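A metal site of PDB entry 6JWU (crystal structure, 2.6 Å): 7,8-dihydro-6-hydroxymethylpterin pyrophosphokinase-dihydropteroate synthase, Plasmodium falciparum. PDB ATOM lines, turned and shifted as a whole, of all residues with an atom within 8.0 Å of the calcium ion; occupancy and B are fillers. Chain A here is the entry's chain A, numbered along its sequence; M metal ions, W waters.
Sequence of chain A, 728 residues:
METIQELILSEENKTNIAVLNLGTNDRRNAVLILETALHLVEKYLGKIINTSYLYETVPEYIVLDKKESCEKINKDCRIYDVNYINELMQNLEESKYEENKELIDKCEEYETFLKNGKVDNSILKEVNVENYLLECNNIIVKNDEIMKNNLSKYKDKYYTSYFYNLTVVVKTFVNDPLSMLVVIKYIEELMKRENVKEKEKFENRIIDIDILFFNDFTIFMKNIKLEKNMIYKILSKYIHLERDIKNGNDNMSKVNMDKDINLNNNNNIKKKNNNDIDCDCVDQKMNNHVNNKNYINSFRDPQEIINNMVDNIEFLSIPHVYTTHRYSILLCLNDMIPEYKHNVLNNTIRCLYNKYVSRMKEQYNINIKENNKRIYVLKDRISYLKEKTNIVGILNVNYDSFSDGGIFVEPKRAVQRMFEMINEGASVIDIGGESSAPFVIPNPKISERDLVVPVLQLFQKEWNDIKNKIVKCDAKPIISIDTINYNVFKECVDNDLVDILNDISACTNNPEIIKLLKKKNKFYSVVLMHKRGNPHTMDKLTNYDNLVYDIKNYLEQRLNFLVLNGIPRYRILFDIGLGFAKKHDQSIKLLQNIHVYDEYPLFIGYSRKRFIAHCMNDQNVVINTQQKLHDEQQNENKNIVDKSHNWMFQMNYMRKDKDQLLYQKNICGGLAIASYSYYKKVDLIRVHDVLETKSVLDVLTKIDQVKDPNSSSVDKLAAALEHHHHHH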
ATOM      1  N   LEU A  38     -15.402  31.069  16.298  1.00  0.00           N
ATOM      2  CA  LEU A  38     -13.923  30.985  16.567  1.00  0.00           C
ATOM      3  C   LEU A  38     -13.684  30.448  17.979  1.00  0.00           C
ATOM      4  O   LEU A  38     -12.816  29.602  18.108  1.00  0.00           O
ATOM      5  CB  LEU A  38     -13.256  32.350  16.375  1.00  0.00           C
ATOM      6  CG  LEU A  38     -13.054  32.803  14.927  1.00  0.00           C
ATOM      7  CD1 LEU A  38     -12.326  34.134  14.883  1.00  0.00           C
ATOM      8  CD2 LEU A  38     -12.287  31.784  14.106  1.00  0.00           C
ATOM      9  N   HIS A  39     -14.441  30.889  18.984  1.00  0.00           N
ATOM     10  CA  HIS A  39     -14.255  30.417  20.395  1.00  0.00           C
ATOM     11  C   HIS A  39     -14.681  28.955  20.531  1.00  0.00           C
ATOM     12  O   HIS A  39     -14.011  28.252  21.285  1.00  0.00           O
ATOM     13  CB  HIS A  39     -14.964  31.302  21.423  1.00  0.00           C
ATOM     14  CG  HIS A  39     -15.097  30.615  22.753  1.00  0.00           C
ATOM     15  ND1 HIS A  39     -14.009  30.278  23.562  1.00  0.00           N
ATOM     16  CD2 HIS A  39     -16.193  30.183  23.422  1.00  0.00           C
ATOM     17  CE1 HIS A  39     -14.442  29.695  24.665  1.00  0.00           C
ATOM     18  NE2 HIS A  39     -15.765  29.623  24.603  1.00  0.00           N
ATOM     19  N   LEU A  40     -15.735  28.518  19.850  1.00  0.00           N
ATOM     20  CA  LEU A  40     -16.187  27.106  19.921  1.00  0.00           C
ATOM     21  C   LEU A  40     -15.171  26.222  19.179  1.00  0.00           C
ATOM     22  O   LEU A  40     -14.957  25.077  19.613  1.00  0.00           O
ATOM     23  CB  LEU A  40     -17.612  26.989  19.374  1.00  0.00           C
ATOM     24  CG  LEU A  40     -18.663  27.810  20.138  1.00  0.00           C
ATOM     25  CD1 LEU A  40     -20.022  27.744  19.459  1.00  0.00           C
ATOM     26  CD2 LEU A  40     -18.813  27.335  21.570  1.00  0.00           C
ATOM     27  N   VAL A  41     -14.495  26.744  18.161  1.00  0.00           N
ATOM     28  CA  VAL A  41     -13.382  26.009  17.482  1.00  0.00           C
ATOM     29  C   VAL A  41     -12.208  25.857  18.462  1.00  0.00           C
ATOM     30  O   VAL A  41     -11.686  24.738  18.528  1.00  0.00           O
ATOM     31  CB  VAL A  41     -12.955  26.685  16.161  1.00  0.00           C
ATOM     32  CG1 VAL A  41     -11.622  26.160  15.665  1.00  0.00           C
ATOM     33  CG2 VAL A  41     -14.014  26.522  15.090  1.00  0.00           C
ATOM     34  N   GLU A  42     -11.768  26.900  19.169  1.00  0.00           N
ATOM     35  CA  GLU A  42     -10.649  26.795  20.168  1.00  0.00           C
ATOM     36  C   GLU A  42     -11.034  25.818  21.280  1.00  0.00           C
ATOM     37  O   GLU A  42     -10.144  25.172  21.869  1.00  0.00           O
ATOM     38  CB  GLU A  42     -10.356  28.110  20.909  1.00  0.00           C
ATOM     39  CG  GLU A  42      -9.252  28.962  20.286  1.00  0.00           C
ATOM     40  CD  GLU A  42      -7.807  28.482  20.430  1.00  0.00           C
ATOM     41  OE1 GLU A  42      -7.528  27.542  21.244  1.00  0.00           O
ATOM     42  OE2 GLU A  42      -6.959  29.051  19.685  1.00  0.00           O
ATOM     43  N   LYS A  43     -12.328  25.798  21.610  1.00  0.00           N
ATOM     44  CA  LYS A  43     -12.823  25.067  22.796  1.00  0.00           C
ATOM     45  C   LYS A  43     -12.951  23.587  22.456  1.00  0.00           C
ATOM     46  O   LYS A  43     -12.474  22.767  23.269  1.00  0.00           O
ATOM     47  CB  LYS A  43     -14.144  25.692  23.253  1.00  0.00           C
ATOM     48  CG  LYS A  43     -14.735  25.093  24.519  1.00  0.00           C
ATOM     49  CD  LYS A  43     -16.010  25.818  24.921  1.00  0.00           C
ATOM     50  CE  LYS A  43     -16.774  25.163  26.056  1.00  0.00           C
ATOM     51  NZ  LYS A  43     -16.001  25.183  27.327  1.00  0.00           N
ATOM     52  N   TYR A  44     -13.531  23.261  21.295  1.00  0.00           N
ATOM     53  CA  TYR A  44     -14.005  21.895  20.983  1.00  0.00           C
ATOM     54  C   TYR A  44     -13.088  21.210  19.965  1.00  0.00           C
ATOM     55  O   TYR A  44     -13.037  19.972  20.028  1.00  0.00           O
ATOM     56  CB  TYR A  44     -15.466  21.911  20.537  1.00  0.00           C
ATOM     57  CG  TYR A  44     -16.461  22.228  21.636  1.00  0.00           C
ATOM     58  CD1 TYR A  44     -16.269  21.788  22.928  1.00  0.00           C
ATOM     59  CD2 TYR A  44     -17.616  22.954  21.367  1.00  0.00           C
ATOM     60  CE1 TYR A  44     -17.175  22.075  23.929  1.00  0.00           C
ATOM     61  CE2 TYR A  44     -18.527  23.256  22.351  1.00  0.00           C
ATOM     62  CZ  TYR A  44     -18.308  22.819  23.650  1.00  0.00           C
ATOM     63  OH  TYR A  44     -19.211  23.136  24.651  1.00  0.00           O
ATOM     64  N   LEU A  45     -12.368  21.903  19.086  1.00  0.00           N
ATOM     65  CA  LEU A  45     -11.680  21.200  17.967  1.00  0.00           C
ATOM     66  C   LEU A  45     -10.165  21.181  18.184  1.00  0.00           C
ATOM     67  O   LEU A  45      -9.527  20.206  17.744  1.00  0.00           O
ATOM     68  CB  LEU A  45     -12.052  21.840  16.620  1.00  0.00           C
ATOM     69  CG  LEU A  45     -13.534  21.777  16.293  1.00  0.00           C
ATOM     70  CD1 LEU A  45     -13.844  22.493  14.982  1.00  0.00           C
ATOM     71  CD2 LEU A  45     -14.004  20.343  16.217  1.00  0.00           C
ATOM     72  N   GLY A  46      -9.599  22.179  18.853  1.00  0.00           N
ATOM     73  CA  GLY A  46      -8.149  22.207  19.069  1.00  0.00           C
ATOM     74  C   GLY A  46      -7.634  23.615  19.205  1.00  0.00           C
ATOM     75  O   GLY A  46      -8.205  24.373  19.971  1.00  0.00           O
ATOM     76  N   LYS A  47      -6.584  23.955  18.478  1.00  0.00           N
ATOM     77  CA  LYS A  47      -5.913  25.260  18.632  1.00  0.00           C
ATOM     78  C   LYS A  47      -5.931  25.999  17.294  1.00  0.00           C
ATOM     79  O   LYS A  47      -5.524  25.408  16.290  1.00  0.00           O
ATOM     80  CB  LYS A  47      -4.473  25.048  19.109  1.00  0.00           C
ATOM     81  CG  LYS A  47      -3.824  26.327  19.609  1.00  0.00           C
ATOM     82  CD  LYS A  47      -2.342  26.416  19.344  1.00  0.00           C
ATOM     83  CE  LYS A  47      -1.614  27.317  20.311  1.00  0.00           C
ATOM     84  NZ  LYS A  47      -2.407  28.512  20.701  1.00  0.00           N
ATOM     85  N   ILE A  48      -6.369  27.249  17.290  1.00  0.00           N
ATOM     86  CA  ILE A  48      -6.333  28.157  16.111  1.00  0.00           C
ATOM     87  C   ILE A  48      -4.920  28.732  15.957  1.00  0.00           C
ATOM     88  O   ILE A  48      -4.447  29.432  16.897  1.00  0.00           O
ATOM     89  CB  ILE A  48      -7.407  29.255  16.222  1.00  0.00           C
ATOM     90  CG1 ILE A  48      -8.802  28.613  16.259  1.00  0.00           C
ATOM     91  CG2 ILE A  48      -7.272  30.269  15.092  1.00  0.00           C
ATOM     92  CD1 ILE A  48      -9.920  29.552  16.606  1.00  0.00           C
ATOM     93  N   SER A  95     -15.104  20.844  27.126  1.00  0.00           N
ATOM     94  CA  SER A  95     -14.277  19.964  26.260  1.00  0.00           C
ATOM     95  C   SER A  95     -13.596  18.954  27.201  1.00  0.00           C
ATOM     96  O   SER A  95     -13.426  19.308  28.365  1.00  0.00           O
ATOM     97  CB  SER A  95     -13.279  20.741  25.434  1.00  0.00           C
ATOM     98  OG  SER A  95     -12.232  19.899  24.973  1.00  0.00           O
ATOM     99  N   TYR A  97     -10.700  17.896  26.234  1.00  0.00           N
ATOM    100  CA  TYR A  97      -9.316  18.312  25.904  1.00  0.00           C
ATOM    101  C   TYR A  97      -9.078  19.682  26.521  1.00  0.00           C
ATOM    102  O   TYR A  97     -10.000  20.504  26.604  1.00  0.00           O
ATOM    103  CB  TYR A  97      -9.076  18.281  24.404  1.00  0.00           C
ATOM    104  CG  TYR A  97      -9.109  16.894  23.827  1.00  0.00           C
ATOM    105  CD1 TYR A  97     -10.330  16.244  23.658  1.00  0.00           C
ATOM    106  CD2 TYR A  97      -7.952  16.212  23.514  1.00  0.00           C
ATOM    107  CE1 TYR A  97     -10.377  14.954  23.168  1.00  0.00           C
ATOM    108  CE2 TYR A  97      -8.000  14.929  23.001  1.00  0.00           C
ATOM    109  CZ  TYR A  97      -9.217  14.292  22.835  1.00  0.00           C
ATOM    110  OH  TYR A  97      -9.313  13.035  22.321  1.00  0.00           O
ATOM    111  N   GLU A  98      -7.843  19.884  26.966  1.00  0.00           N
ATOM    112  CA  GLU A  98      -7.448  21.027  27.820  1.00  0.00           C
ATOM    113  C   GLU A  98      -7.163  22.231  26.926  1.00  0.00           C
ATOM    114  O   GLU A  98      -6.640  22.020  25.829  1.00  0.00           O
ATOM    115  CB  GLU A  98      -6.176  20.646  28.569  1.00  0.00           C
ATOM    116  CG  GLU A  98      -4.966  20.580  27.653  1.00  0.00           C
ATOM    117  CD  GLU A  98      -4.004  19.476  27.998  1.00  0.00           C
ATOM    118  OE1 GLU A  98      -4.121  18.990  29.140  1.00  0.00           O
ATOM    119  OE2 GLU A  98      -3.155  19.099  27.142  1.00  0.00           O
ATOM    120  N   GLU A  99      -7.464  23.428  27.405  1.00  0.00           N
ATOM    121  CA  GLU A  99      -6.966  24.657  26.748  1.00  0.00           C
ATOM    122  C   GLU A  99      -5.519  24.864  27.197  1.00  0.00           C
ATOM    123  O   GLU A  99      -5.171  24.412  28.295  1.00  0.00           O
ATOM    124  CB  GLU A  99      -7.852  25.868  27.040  1.00  0.00           C
ATOM    125  CG  GLU A  99      -7.632  26.994  26.037  1.00  0.00           C
ATOM    126  CD  GLU A  99      -7.820  26.590  24.575  1.00  0.00           C
ATOM    127  OE1 GLU A  99      -8.972  26.634  24.118  1.00  0.00           O
ATOM    128  OE2 GLU A  99      -6.799  26.214  23.905  1.00  0.00           O
ATOM    129  N   ASN A 100      -4.705  25.468  26.342  1.00  0.00           N
ATOM    130  CA  ASN A 100      -3.327  25.900  26.635  1.00  0.00           C
ATOM    131  C   ASN A 100      -3.149  27.255  25.961  1.00  0.00           C
ATOM    132  O   ASN A 100      -3.106  27.277  24.731  1.00  0.00           O
ATOM    133  CB  ASN A 100      -2.305  24.894  26.125  1.00  0.00           C
ATOM    134  CG  ASN A 100      -2.328  23.617  26.930  1.00  0.00           C
ATOM    135  OD1 ASN A 100      -2.403  23.669  28.159  1.00  0.00           O
ATOM    136  ND2 ASN A 100      -2.255  22.483  26.251  1.00  0.00           N
ATOM    137  N   LYS A 101      -3.124  28.322  26.747  1.00  0.00           N
ATOM    138  CA  LYS A 101      -2.944  29.697  26.247  1.00  0.00           C
ATOM    139  C   LYS A 101      -1.451  30.020  26.131  1.00  0.00           C
ATOM    140  O   LYS A 101      -1.146  31.088  25.669  1.00  0.00           O
ATOM    141  CB  LYS A 101      -3.727  30.649  27.160  1.00  0.00           C
ATOM    142  CG  LYS A 101      -5.241  30.516  27.041  1.00  0.00           C
ATOM    143  CD  LYS A 101      -6.078  31.434  27.924  1.00  0.00           C
ATOM    144  CE  LYS A 101      -5.683  32.899  27.878  1.00  0.00           C
ATOM    145  NZ  LYS A 101      -5.984  33.523  26.576  1.00  0.00           N
ATOM    146  N   VAL A 170      -6.666  25.064  12.091  1.00  0.00           N
ATOM    147  CA  VAL A 170      -6.809  24.441  13.425  1.00  0.00           C
ATOM    148  C   VAL A 170      -5.815  23.289  13.533  1.00  0.00           C
ATOM    149  O   VAL A 170      -5.806  22.437  12.656  1.00  0.00           O
ATOM    150  CB  VAL A 170      -8.230  23.923  13.667  1.00  0.00           C
ATOM    151  CG1 VAL A 170      -8.430  23.480  15.105  1.00  0.00           C
ATOM    152  CG2 VAL A 170      -9.244  24.977  13.294  1.00  0.00           C
ATOM    153  N   LYS A 171      -5.005  23.300  14.588  1.00  0.00           N
ATOM    154  CA  LYS A 171      -4.270  22.116  15.074  1.00  0.00           C
ATOM    155  C   LYS A 171      -5.256  21.394  15.968  1.00  0.00           C
ATOM    156  O   LYS A 171      -5.521  21.917  17.053  1.00  0.00           O
ATOM    157  CB  LYS A 171      -2.991  22.533  15.806  1.00  0.00           C
ATOM    158  CG  LYS A 171      -2.095  21.386  16.199  1.00  0.00           C
ATOM    159  CD  LYS A 171      -1.144  21.725  17.313  1.00  0.00           C
ATOM    160  CE  LYS A 171       0.241  22.106  16.826  1.00  0.00           C
ATOM    161  NZ  LYS A 171       0.946  23.007  17.770  1.00  0.00           N
ATOM    162  N   PHE A 173      -7.175  17.928  17.853  1.00  0.00           N
ATOM    163  CA  PHE A 173      -7.054  16.628  18.544  1.00  0.00           C
ATOM    164  C   PHE A 173      -8.126  15.664  18.013  1.00  0.00           C
ATOM    165  O   PHE A 173      -8.176  14.499  18.452  1.00  0.00           O
ATOM    166  CB  PHE A 173      -7.196  16.782  20.060  1.00  0.00           C
ATOM    167  CG  PHE A 173      -8.285  17.743  20.485  1.00  0.00           C
ATOM    168  CD1 PHE A 173      -9.618  17.429  20.297  1.00  0.00           C
ATOM    169  CD2 PHE A 173      -7.960  18.965  21.065  1.00  0.00           C
ATOM    170  CE1 PHE A 173     -10.603  18.345  20.630  1.00  0.00           C
ATOM    171  CE2 PHE A 173      -8.957  19.863  21.398  1.00  0.00           C
ATOM    172  CZ  PHE A 173     -10.267  19.567  21.171  1.00  0.00           C
ATOM    173  N   LYS A 518      -7.170  37.590  24.139  1.00  0.00           N
ATOM    174  CA  LYS A 518      -8.232  36.544  24.054  1.00  0.00           C
ATOM    175  C   LYS A 518      -8.827  36.393  25.452  1.00  0.00           C
ATOM    176  O   LYS A 518      -8.143  35.854  26.325  1.00  0.00           O
ATOM    177  CB  LYS A 518      -7.713  35.177  23.584  1.00  0.00           C
ATOM    178  CG  LYS A 518      -6.817  35.143  22.363  1.00  0.00           C
ATOM    179  CD  LYS A 518      -5.647  34.148  22.482  1.00  0.00           C
ATOM    180  CE  LYS A 518      -5.937  32.773  21.924  1.00  0.00           C
ATOM    181  NZ  LYS A 518      -5.162  31.702  22.622  1.00  0.00           N
HETATM  182 CA    CA M   1      -8.016  25.222  22.271  1.00  0.00          CA
HETATM  183  O   HOH W   1      -6.011  24.219  21.969  1.00  0.00           O
HETATM  184  O   HOH W   2      -8.345  23.307  23.480  1.00  0.00           O
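N of Ile 48 lies within hydrogen-bond range of OE2 of Glu 42, at 3.1 Å.
O of Val 41 lies within hydrogen-bond range of N of Gly 46, at 3.3 Å.
The nearest printed residue that does not touch the calcium ion is Lys 47 (4.2 Å).
The backbone carbonyl oxygen (O) of Glu 42 is bound to the calcium ion, at 2.2 Å.
The calcium ion is bound by water W1 (2.3 Å).
The side-chain carboxylate (OE2) of Glu 99 is bound to the calcium ion (2.3 Å).
Water W2 is bound to the calcium ion (2.3 Å).
The calcium ion is bound by O of Gly 46 (2.5 Å).
The calcium ion is bound by OE1 of Glu 99, at 2.5 Å.
OE1 of Glu 42 binds the calcium ion, at 2.6 Å.
The calcium ion has seven donor atoms within binding distance.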
